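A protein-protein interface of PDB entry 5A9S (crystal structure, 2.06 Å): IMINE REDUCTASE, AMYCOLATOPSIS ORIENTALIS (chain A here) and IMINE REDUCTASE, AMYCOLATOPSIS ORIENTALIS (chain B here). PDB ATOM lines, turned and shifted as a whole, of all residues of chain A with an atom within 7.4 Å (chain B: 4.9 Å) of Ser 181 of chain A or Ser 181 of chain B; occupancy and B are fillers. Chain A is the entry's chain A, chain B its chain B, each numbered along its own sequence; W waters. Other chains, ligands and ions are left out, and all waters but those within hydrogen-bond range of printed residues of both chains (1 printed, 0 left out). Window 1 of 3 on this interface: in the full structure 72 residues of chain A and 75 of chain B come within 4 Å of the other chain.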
ATOM      1  N   LEU A 174      25.710  -1.517  23.403  1.00  0.00           N
ATOM      2  CA  LEU A 174      26.031  -2.491  24.418  1.00  0.00           C
ATOM      3  C   LEU A 174      25.005  -3.632  24.374  1.00  0.00           C
ATOM      4  O   LEU A 174      25.349  -4.811  24.442  1.00  0.00           O
ATOM      5  CB  LEU A 174      26.073  -1.828  25.823  1.00  0.00           C
ATOM      6  CG  LEU A 174      27.238  -0.861  26.034  1.00  0.00           C
ATOM      7  CD1 LEU A 174      27.034  -0.021  27.295  1.00  0.00           C
ATOM      8  CD2 LEU A 174      28.588  -1.592  26.118  1.00  0.00           C
ATOM      9  N   LEU A 175      23.737  -3.280  24.251  1.00  0.00           N
ATOM     10  CA  LEU A 175      22.722  -4.281  24.172  1.00  0.00           C
ATOM     11  C   LEU A 175      22.804  -5.146  22.900  1.00  0.00           C
ATOM     12  O   LEU A 175      22.491  -6.334  22.946  1.00  0.00           O
ATOM     13  CB  LEU A 175      21.332  -3.657  24.257  1.00  0.00           C
ATOM     14  CG  LEU A 175      20.936  -3.028  25.549  1.00  0.00           C
ATOM     15  CD1 LEU A 175      19.631  -2.232  25.408  1.00  0.00           C
ATOM     16  CD2 LEU A 175      20.747  -4.091  26.630  1.00  0.00           C
ATOM     17  N   SER A 176      23.216  -4.578  21.788  1.00  0.00           N
ATOM     18  CA  SER A 176      23.459  -5.367  20.599  1.00  0.00           C
ATOM     19  C   SER A 176      24.531  -6.478  20.845  1.00  0.00           C
ATOM     20  O   SER A 176      24.368  -7.616  20.451  1.00  0.00           O
ATOM     21  CB  SER A 176      23.887  -4.470  19.446  1.00  0.00           C
ATOM     22  OG  SER A 176      23.839  -5.185  18.239  1.00  0.00           O
ATOM     23  N   MET A 177      25.612  -6.119  21.523  1.00  0.00           N
ATOM     24  CA  MET A 177      26.633  -7.098  21.951  1.00  0.00           C
ATOM     25  C   MET A 177      26.020  -8.169  22.869  1.00  0.00           C
ATOM     26  O   MET A 177      26.328  -9.337  22.752  1.00  0.00           O
ATOM     27  CB  MET A 177      27.720  -6.362  22.679  1.00  0.00           C
ATOM     28  CG  MET A 177      28.934  -7.212  23.117  1.00  0.00           C
ATOM     29  SD  MET A 177      30.051  -6.232  24.205  1.00  0.00           S
ATOM     30  CE  MET A 177      31.179  -7.543  24.675  1.00  0.00           C
ATOM     31  N   MET A 178      25.174  -7.737  23.798  1.00  0.00           N
ATOM     32  CA  MET A 178      24.572  -8.654  24.773  1.00  0.00           C
ATOM     33  C   MET A 178      23.762  -9.734  24.070  1.00  0.00           C
ATOM     34  O   MET A 178      23.881 -10.898  24.453  1.00  0.00           O
ATOM     35  CB  MET A 178      23.691  -7.904  25.789  1.00  0.00           C
ATOM     36  CG  MET A 178      22.978  -8.792  26.800  1.00  0.00           C
ATOM     37  SD  MET A 178      21.762  -7.820  27.739  1.00  0.00           S
ATOM     38  CE  MET A 178      20.441  -7.901  26.518  1.00  0.00           C
ATOM     39  N   TYR A 179      22.909  -9.336  23.120  1.00  0.00           N
ATOM     40  CA  TYR A 179      22.069 -10.315  22.433  1.00  0.00           C
ATOM     41  C   TYR A 179      22.927 -11.332  21.694  1.00  0.00           C
ATOM     42  O   TYR A 179      22.673 -12.542  21.791  1.00  0.00           O
ATOM     43  CB  TYR A 179      21.008  -9.674  21.524  1.00  0.00           C
ATOM     44  CG  TYR A 179      19.930  -8.928  22.299  1.00  0.00           C
ATOM     45  CD1 TYR A 179      19.046  -9.622  23.164  1.00  0.00           C
ATOM     46  CD2 TYR A 179      19.776  -7.528  22.213  1.00  0.00           C
ATOM     47  CE1 TYR A 179      18.073  -8.931  23.899  1.00  0.00           C
ATOM     48  CE2 TYR A 179      18.800  -6.858  22.948  1.00  0.00           C
ATOM     49  CZ  TYR A 179      17.970  -7.550  23.794  1.00  0.00           C
ATOM     50  OH  TYR A 179      17.000  -6.891  24.502  1.00  0.00           O
ATOM     51  N   SER A 180      23.947 -10.860  20.983  1.00  0.00           N
ATOM     52  CA  SER A 180      24.822 -11.777  20.236  1.00  0.00           C
ATOM     53  C   SER A 180      25.513 -12.710  21.143  1.00  0.00           C
ATOM     54  O   SER A 180      25.593 -13.909  20.848  1.00  0.00           O
ATOM     55  CB  SER A 180      25.844 -11.016  19.437  1.00  0.00           C
ATOM     56  OG  SER A 180      25.222 -10.287  18.401  1.00  0.00           O
ATOM     57  N   SER A 181      26.002 -12.185  22.275  1.00  0.00           N
ATOM     58  CA  SER A 181      26.735 -12.998  23.255  1.00  0.00           C
ATOM     59  C   SER A 181      25.839 -14.036  23.905  1.00  0.00           C
ATOM     60  O   SER A 181      26.228 -15.191  24.110  1.00  0.00           O
ATOM     61  CB  SER A 181      27.354 -12.141  24.373  1.00  0.00           C
ATOM     62  OG  SER A 181      28.130 -11.089  23.869  1.00  0.00           O
ATOM     63  N   MET A 182      24.622 -13.652  24.193  1.00  0.00           N
ATOM     64  CA  MET A 182      23.683 -14.591  24.797  1.00  0.00           C
ATOM     65  C   MET A 182      23.317 -15.703  23.839  1.00  0.00           C
ATOM     66  O   MET A 182      23.149 -16.848  24.261  1.00  0.00           O
ATOM     67  CB  MET A 182      22.397 -13.898  25.267  1.00  0.00           C
ATOM     68  CG  MET A 182      22.628 -13.113  26.541  1.00  0.00           C
ATOM     69  SD  MET A 182      21.181 -12.334  27.256  1.00  0.00           S
ATOM     70  CE  MET A 182      20.196 -11.633  25.939  1.00  0.00           C
ATOM     71  N   ASN A 183      23.140 -15.358  22.572  1.00  0.00           N
ATOM     72  CA  ASN A 183      22.799 -16.364  21.575  1.00  0.00           C
ATOM     73  C   ASN A 183      23.928 -17.353  21.361  1.00  0.00           C
ATOM     74  O   ASN A 183      23.678 -18.537  21.243  1.00  0.00           O
ATOM     75  CB  ASN A 183      22.380 -15.709  20.241  1.00  0.00           C
ATOM     76  CG  ASN A 183      21.146 -14.831  20.369  1.00  0.00           C
ATOM     77  OD1 ASN A 183      20.902 -13.930  19.536  1.00  0.00           O
ATOM     78  ND2 ASN A 183      20.409 -15.029  21.422  1.00  0.00           N
ATOM     79  N   GLY A 184      25.178 -16.865  21.379  1.00  0.00           N
ATOM     80  CA  GLY A 184      26.323 -17.717  21.336  1.00  0.00           C
ATOM     81  C   GLY A 184      26.428 -18.644  22.532  1.00  0.00           C
ATOM     82  O   GLY A 184      26.720 -19.860  22.386  1.00  0.00           O
ATOM     83  N   PHE A 185      26.189 -18.081  23.712  1.00  0.00           N
ATOM     84  CA  PHE A 185      26.109 -18.868  24.941  1.00  0.00           C
ATOM     85  C   PHE A 185      25.070 -19.981  24.822  1.00  0.00           C
ATOM     86  O   PHE A 185      25.309 -21.075  25.211  1.00  0.00           O
ATOM     87  CB  PHE A 185      25.762 -18.033  26.200  1.00  0.00           C
ATOM     88  CG  PHE A 185      25.536 -18.899  27.385  1.00  0.00           C
ATOM     89  CD1 PHE A 185      26.629 -19.486  28.034  1.00  0.00           C
ATOM     90  CD2 PHE A 185      24.262 -19.278  27.742  1.00  0.00           C
ATOM     91  CE1 PHE A 185      26.442 -20.378  29.048  1.00  0.00           C
ATOM     92  CE2 PHE A 185      24.076 -20.193  28.764  1.00  0.00           C
ATOM     93  CZ  PHE A 185      25.161 -20.720  29.421  1.00  0.00           C
ATOM     94  N   LEU A 186      23.890 -19.658  24.304  1.00  0.00           N
ATOM     95  CA  LEU A 186      22.835 -20.663  24.191  1.00  0.00           C
ATOM     96  C   LEU A 186      23.232 -21.791  23.240  1.00  0.00           C
ATOM     97  O   LEU A 186      22.978 -22.924  23.522  1.00  0.00           O
ATOM     98  CB  LEU A 186      21.499 -20.025  23.797  1.00  0.00           C
ATOM     99  CG  LEU A 186      20.895 -19.101  24.875  1.00  0.00           C
ATOM    100  CD1 LEU A 186      19.661 -18.512  24.272  1.00  0.00           C
ATOM    101  CD2 LEU A 186      20.533 -19.814  26.208  1.00  0.00           C
ATOM    102  N   HIS A 187      23.918 -21.472  22.152  1.00  0.00           N
ATOM    103  CA  HIS A 187      24.438 -22.504  21.306  1.00  0.00           C
ATOM    104  C   HIS A 187      25.467 -23.382  22.029  1.00  0.00           C
ATOM    105  O   HIS A 187      25.390 -24.627  21.962  1.00  0.00           O
ATOM    106  CB  HIS A 187      25.042 -21.957  20.036  1.00  0.00           C
ATOM    107  CG  HIS A 187      25.526 -23.038  19.140  1.00  0.00           C
ATOM    108  ND1 HIS A 187      26.863 -23.335  18.971  1.00  0.00           N
ATOM    109  CD2 HIS A 187      24.833 -23.943  18.407  1.00  0.00           C
ATOM    110  CE1 HIS A 187      26.969 -24.382  18.167  1.00  0.00           C
ATOM    111  NE2 HIS A 187      25.747 -24.754  17.799  1.00  0.00           N
ATOM    112  N   PHE A 210      35.553 -17.938  31.342  1.00  0.00           N
ATOM    113  CA  PHE A 210      35.852 -17.762  29.932  1.00  0.00           C
ATOM    114  C   PHE A 210      35.510 -16.384  29.434  1.00  0.00           C
ATOM    115  O   PHE A 210      36.241 -15.777  28.646  1.00  0.00           O
ATOM    116  CB  PHE A 210      35.124 -18.825  29.125  1.00  0.00           C
ATOM    117  CG  PHE A 210      35.508 -18.847  27.690  1.00  0.00           C
ATOM    118  CD1 PHE A 210      36.715 -19.433  27.309  1.00  0.00           C
ATOM    119  CD2 PHE A 210      34.664 -18.328  26.718  1.00  0.00           C
ATOM    120  CE1 PHE A 210      37.061 -19.524  25.975  1.00  0.00           C
ATOM    121  CE2 PHE A 210      35.012 -18.394  25.381  1.00  0.00           C
ATOM    122  CZ  PHE A 210      36.217 -18.984  25.012  1.00  0.00           C
ATOM    123  N   LEU A 211      34.351 -15.896  29.862  1.00  0.00           N
ATOM    124  CA  LEU A 211      33.876 -14.606  29.438  1.00  0.00           C
ATOM    125  C   LEU A 211      34.883 -13.456  29.706  1.00  0.00           C
ATOM    126  O   LEU A 211      35.299 -12.779  28.793  1.00  0.00           O
ATOM    127  CB  LEU A 211      32.467 -14.386  30.009  1.00  0.00           C
ATOM    128  CG  LEU A 211      31.678 -13.133  29.666  1.00  0.00           C
ATOM    129  CD1 LEU A 211      31.507 -13.130  28.148  1.00  0.00           C
ATOM    130  CD2 LEU A 211      30.271 -13.064  30.299  1.00  0.00           C
ATOM    131  N   ILE A 215      37.133 -14.069  26.323  1.00  0.00           N
ATOM    132  CA  ILE A 215      36.377 -13.227  25.412  1.00  0.00           C
ATOM    133  C   ILE A 215      36.824 -11.750  25.575  1.00  0.00           C
ATOM    134  O   ILE A 215      37.157 -11.114  24.604  1.00  0.00           O
ATOM    135  CB  ILE A 215      34.836 -13.392  25.569  1.00  0.00           C
ATOM    136  CG1 ILE A 215      34.461 -14.833  25.173  1.00  0.00           C
ATOM    137  CG2 ILE A 215      34.082 -12.368  24.754  1.00  0.00           C
ATOM    138  CD1 ILE A 215      32.987 -15.165  25.308  1.00  0.00           C
ATOM    139  N   GLY A 216      36.829 -11.251  26.808  1.00  0.00           N
ATOM    140  CA  GLY A 216      37.210  -9.886  27.057  1.00  0.00           C
ATOM    141  C   GLY A 216      38.635  -9.547  26.658  1.00  0.00           C
ATOM    142  O   GLY A 216      38.885  -8.465  26.106  1.00  0.00           O
ATOM    143  N   ILE A 219      38.882  -9.472  22.747  1.00  0.00           N
ATOM    144  CA  ILE A 219      38.351  -8.233  22.258  1.00  0.00           C
ATOM    145  C   ILE A 219      39.369  -7.136  22.445  1.00  0.00           C
ATOM    146  O   ILE A 219      39.647  -6.397  21.523  1.00  0.00           O
ATOM    147  CB  ILE A 219      37.018  -7.861  22.962  1.00  0.00           C
ATOM    148  CG1 ILE A 219      35.938  -8.773  22.437  1.00  0.00           C
ATOM    149  CG2 ILE A 219      36.675  -6.388  22.726  1.00  0.00           C
ATOM    150  CD1 ILE A 219      34.645  -8.712  23.224  1.00  0.00           C
ATOM    151  N   ASN A 265      28.032 -17.388  11.679  1.00  0.00           N
ATOM    152  CA  ASN A 265      29.352 -16.792  12.018  1.00  0.00           C
ATOM    153  C   ASN A 265      30.411 -17.055  10.967  1.00  0.00           C
ATOM    154  O   ASN A 265      31.200 -16.195  10.604  1.00  0.00           O
ATOM    155  CB  ASN A 265      29.796 -17.290  13.418  1.00  0.00           C
ATOM    156  CG  ASN A 265      29.013 -16.629  14.528  1.00  0.00           C
ATOM    157  OD1 ASN A 265      28.519 -15.553  14.338  1.00  0.00           O
ATOM    158  ND2 ASN A 265      28.898 -17.250  15.656  1.00  0.00           N
ATOM    159  N   TYR A 282      40.951 -10.271  12.673  1.00  0.00           N
ATOM    160  CA  TYR A 282      39.516 -10.552  12.943  1.00  0.00           C
ATOM    161  C   TYR A 282      38.743  -9.226  12.992  1.00  0.00           C
ATOM    162  O   TYR A 282      37.668  -9.124  12.449  1.00  0.00           O
ATOM    163  CB  TYR A 282      39.290 -11.324  14.281  1.00  0.00           C
ATOM    164  CG  TYR A 282      37.868 -11.935  14.332  1.00  0.00           C
ATOM    165  CD1 TYR A 282      36.767 -11.181  14.696  1.00  0.00           C
ATOM    166  CD2 TYR A 282      37.649 -13.260  14.023  1.00  0.00           C
ATOM    167  CE1 TYR A 282      35.482 -11.699  14.669  1.00  0.00           C
ATOM    168  CE2 TYR A 282      36.381 -13.801  13.999  1.00  0.00           C
ATOM    169  CZ  TYR A 282      35.300 -13.021  14.344  1.00  0.00           C
ATOM    170  OH  TYR A 282      34.063 -13.565  14.363  1.00  0.00           O
ATOM    171  N   MET B 177      30.522 -19.402  21.471  1.00  0.00           N
ATOM    172  CA  MET B 177      30.167 -18.226  22.209  1.00  0.00           C
ATOM    173  C   MET B 177      31.086 -17.054  21.939  1.00  0.00           C
ATOM    174  O   MET B 177      30.621 -15.917  21.799  1.00  0.00           O
ATOM    175  CB  MET B 177      30.147 -18.559  23.713  1.00  0.00           C
ATOM    176  CG  MET B 177      29.694 -17.468  24.665  1.00  0.00           C
ATOM    177  SD  MET B 177      29.948 -17.941  26.392  1.00  0.00           S
ATOM    178  CE  MET B 177      29.478 -16.387  27.180  1.00  0.00           C
ATOM    179  N   MET B 178      32.393 -17.330  21.874  1.00  0.00           N
ATOM    180  CA  MET B 178      33.380 -16.285  21.631  1.00  0.00           C
ATOM    181  C   MET B 178      33.166 -15.597  20.311  1.00  0.00           C
ATOM    182  O   MET B 178      33.173 -14.355  20.286  1.00  0.00           O
ATOM    183  CB  MET B 178      34.781 -16.849  21.704  1.00  0.00           C
ATOM    184  CG  MET B 178      35.869 -15.835  21.421  1.00  0.00           C
ATOM    185  SD  MET B 178      37.463 -16.672  21.239  1.00  0.00           S
ATOM    186  CE  MET B 178      37.243 -17.102  19.482  1.00  0.00           C
ATOM    187  N   TYR B 179      32.972 -16.362  19.218  1.00  0.00           N
ATOM    188  CA  TYR B 179      32.723 -15.741  17.943  1.00  0.00           C
ATOM    189  C   TYR B 179      31.479 -14.885  17.938  1.00  0.00           C
ATOM    190  O   TYR B 179      31.507 -13.710  17.451  1.00  0.00           O
ATOM    191  CB  TYR B 179      32.708 -16.753  16.760  1.00  0.00           C
ATOM    192  CG  TYR B 179      34.068 -17.374  16.512  1.00  0.00           C
ATOM    193  CD1 TYR B 179      35.148 -16.597  16.077  1.00  0.00           C
ATOM    194  CD2 TYR B 179      34.296 -18.740  16.746  1.00  0.00           C
ATOM    195  CE1 TYR B 179      36.391 -17.175  15.836  1.00  0.00           C
ATOM    196  CE2 TYR B 179      35.526 -19.311  16.496  1.00  0.00           C
ATOM    197  CZ  TYR B 179      36.571 -18.526  16.067  1.00  0.00           C
ATOM    198  OH  TYR B 179      37.774 -19.092  15.867  1.00  0.00           O
ATOM    199  N   SER B 180      30.386 -15.387  18.511  1.00  0.00           N
ATOM    200  CA  SER B 180      29.149 -14.582  18.535  1.00  0.00           C
ATOM    201  C   SER B 180      29.344 -13.302  19.357  1.00  0.00           C
ATOM    202  O   SER B 180      28.873 -12.244  18.938  1.00  0.00           O
ATOM    203  CB  SER B 180      28.003 -15.383  19.123  1.00  0.00           C
ATOM    204  OG  SER B 180      27.681 -16.485  18.322  1.00  0.00           O
ATOM    205  N   SER B 181      30.006 -13.403  20.526  1.00  0.00           N
ATOM    206  CA  SER B 181      30.248 -12.251  21.381  1.00  0.00           C
ATOM    207  C   SER B 181      31.121 -11.214  20.687  1.00  0.00           C
ATOM    208  O   SER B 181      30.867  -9.998  20.819  1.00  0.00           O
ATOM    209  CB  SER B 181      30.927 -12.631  22.689  1.00  0.00           C
ATOM    210  OG  SER B 181      30.214 -13.670  23.310  1.00  0.00           O
ATOM    211  N   MET B 182      32.134 -11.686  19.940  1.00  0.00           N
ATOM    212  CA  MET B 182      33.055 -10.788  19.223  1.00  0.00           C
ATOM    213  C   MET B 182      32.347 -10.073  18.122  1.00  0.00           C
ATOM    214  O   MET B 182      32.540  -8.873  17.936  1.00  0.00           O
ATOM    215  CB  MET B 182      34.258 -11.502  18.644  1.00  0.00           C
ATOM    216  CG  MET B 182      35.282 -11.929  19.655  1.00  0.00           C
ATOM    217  SD  MET B 182      36.569 -12.983  18.873  1.00  0.00           S
ATOM    218  CE  MET B 182      37.299 -11.662  17.918  1.00  0.00           C
ATOM    219  N   ASN B 183      31.468 -10.785  17.440  1.00  0.00           N
ATOM    220  CA  ASN B 183      30.681 -10.165  16.382  1.00  0.00           C
ATOM    221  C   ASN B 183      29.718  -9.111  16.917  1.00  0.00           C
ATOM    222  O   ASN B 183      29.542  -8.067  16.286  1.00  0.00           O
ATOM    223  CB  ASN B 183      29.934 -11.186  15.495  1.00  0.00           C
ATOM    224  CG  ASN B 183      30.864 -12.166  14.801  1.00  0.00           C
ATOM    225  OD1 ASN B 183      30.470 -13.315  14.461  1.00  0.00           O
ATOM    226  ND2 ASN B 183      32.102 -11.794  14.666  1.00  0.00           N
ATOM    227  N   GLY B 184      29.077  -9.390  18.038  1.00  0.00           N
ATOM    228  CA  GLY B 184      28.202  -8.413  18.688  1.00  0.00           C
ATOM    229  C   GLY B 184      28.978  -7.187  19.139  1.00  0.00           C
ATOM    230  O   GLY B 184      28.516  -6.043  18.959  1.00  0.00           O
ATOM    231  N   PHE B 185      30.167  -7.425  19.697  1.00  0.00           N
ATOM    232  CA  PHE B 185      31.071  -6.333  20.076  1.00  0.00           C
ATOM    233  C   PHE B 185      31.395  -5.487  18.876  1.00  0.00           C
ATOM    234  O   PHE B 185      31.396  -4.257  18.944  1.00  0.00           O
ATOM    235  CB  PHE B 185      32.377  -6.786  20.730  1.00  0.00           C
ATOM    236  CG  PHE B 185      33.307  -5.639  20.937  1.00  0.00           C
ATOM    237  CD1 PHE B 185      33.094  -4.750  21.983  1.00  0.00           C
ATOM    238  CD2 PHE B 185      34.256  -5.327  19.979  1.00  0.00           C
ATOM    239  CE1 PHE B 185      33.853  -3.595  22.101  1.00  0.00           C
ATOM    240  CE2 PHE B 185      35.038  -4.196  20.115  1.00  0.00           C
ATOM    241  CZ  PHE B 185      34.843  -3.350  21.183  1.00  0.00           C
ATOM    242  N   ILE B 215      26.271  -8.772  30.990  1.00  0.00           N
ATOM    243  CA  ILE B 215      26.139  -9.963  30.139  1.00  0.00           C
ATOM    244  C   ILE B 215      26.250 -11.233  30.997  1.00  0.00           C
ATOM    245  O   ILE B 215      25.357 -12.060  30.965  1.00  0.00           O
ATOM    246  CB  ILE B 215      27.135  -9.979  28.968  1.00  0.00           C
ATOM    247  CG1 ILE B 215      26.864  -8.792  28.020  1.00  0.00           C
ATOM    248  CG2 ILE B 215      27.089 -11.314  28.206  1.00  0.00           C
ATOM    249  CD1 ILE B 215      27.819  -8.669  26.831  1.00  0.00           C
ATOM    250  N   ILE B 219      23.167 -13.890  31.822  1.00  0.00           N
ATOM    251  CA  ILE B 219      23.264 -15.308  31.467  1.00  0.00           C
ATOM    252  C   ILE B 219      22.976 -16.165  32.691  1.00  0.00           C
ATOM    253  O   ILE B 219      22.165 -17.074  32.624  1.00  0.00           O
ATOM    254  CB  ILE B 219      24.633 -15.651  30.925  1.00  0.00           C
ATOM    255  CG1 ILE B 219      24.750 -15.108  29.497  1.00  0.00           C
ATOM    256  CG2 ILE B 219      24.864 -17.171  30.910  1.00  0.00           C
ATOM    257  CD1 ILE B 219      26.144 -15.117  28.910  1.00  0.00           C
HETATM  258  O   HOH W   1      32.323 -15.165  13.065  1.00  0.00           O
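OG of Ser 181 of chain B sits at hydrogen-bond distance from OG of Ser 181 of chain A (3.4 Å).
The side-chain amide nitrogen (ND2) of Asn 265 of chain A lies within hydrogen-bond range of the side-chain hydroxyl (OG) of Ser 180 of chain B.
The side-chain amide oxygen (OD1) of Asn 265 of chain A lies close to the side-chain amide oxygen (OD1) of Asn 183 of chain B, 3.0 Å away.
The side-chain hydroxyl of Tyr 282 of chain A sits at hydrogen-bond distance from the side-chain amide nitrogen of Asn 183 of chain B (2.7 Å).
The backbone carbonyl oxygen (O) of Ser 176 of chain A lies within hydrogen-bond range of the side-chain hydroxyl (OG) of Ser 180 of chain A (3.5 Å).
The backbone carbonyl oxygen of Met 177 of chain A sits at hydrogen-bond distance from the side-chain hydroxyl of Ser 181 of chain A, at 2.8 Å.
O of Phe 210 of chain A is in hydrogen-bond range of N of Ile 215 of chain A (3.0 Å).
The backbone carbonyl oxygen of Leu 211 of chain A is in hydrogen-bond range of the backbone NH of Gly 216 of chain A (2.9 Å).
O of Met 177 of chain B is in hydrogen-bond range of OG of Ser 181 of chain B.
OD1 of Asn 183 of chain B lies close to O of Tyr 179 of chain B (3.2 Å).
Among the printed residues, pairs that only touch across the chains: Met 177 of chain A with Gly 184 of chain B (3.7 Å), Met 177 of chain A with Phe 185 of chain B (3.6 Å), Met 178 of chain A with Ile 215 of chain B (3.8 Å), Ser 180 of chain A with Ser 180 of chain B (3.3 Å), Ser 180 of chain A with Gly 184 of chain B (3.5 Å), Ser 181 of chain A with Ile 215 of chain B (3.8 Å), Gly 184 of chain A with Met 177 of chain B (3.8 Å), Gly 184 of chain A with Ser 180 of chain B (3.5 Å), Phe 185 of chain A with Met 177 of chain B (3.7 Å), Phe 185 of chain A with Ile 219 of chain B (3.8 Å), Phe 210 of chain A with Met 178 of chain B (3.995 Å), Leu 211 of chain A with Met 177 of chain B (3.96 Å), Ile 215 of chain A with Met 178 of chain B (3.9 Å), Ile 215 of chain A with Ser 181 of chain B (3.7 Å), Ile 219 of chain A with Phe 185 of chain B (3.8 Å), Asn 265 of chain A with Tyr 179 of chain B (3.998 Å), Tyr 282 of chain A with Tyr 179 of chain B (3.6 Å) and Tyr 282 of chain A with Met 182 of chain B (3.3 Å).
Of the printed residues of chain B, Met 177 of chain A touches Gly 184 and Phe 185.
Of the printed residues of chain B, Ser 180 of chain A touches Ser 180 (3.3 Å) and Gly 184 (3.5 Å).
Of the printed residues of chain A, Ser 181 of chain B touches Ser 181 and Ile 215.
Of the printed residues of chain A, Asn 183 of chain B touches Asn 265 (3.0 Å) and Tyr 282 (2.7 Å).
The nearest printed residue of chain A that does not touch Gly 184 of chain B is Ser 176 of chain A (4.3 Å).
Hydrophobic or aromatic side chains of chain B within 4 Å of the printed part of chain A: Met 177, Met 178, Tyr 179, Met 182, Phe 185, Ile 215 and Ile 219.
Hydrophobic or aromatic side chains of chain A within 4 Å of the printed part of chain B: Met 177, Met 178, Phe 185, Phe 210, Leu 211, Ile 215, Ile 219 and Tyr 282.
Water W1 lies within hydrogen-bond range of the side-chain hydroxyl of Tyr 282 of chain A (2.7 Å), the backbone carbonyl oxygen of Asn 265 of chain A (2.9 Å) and the side-chain amide oxygen of Asn 183 of chain B (3.0 Å).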
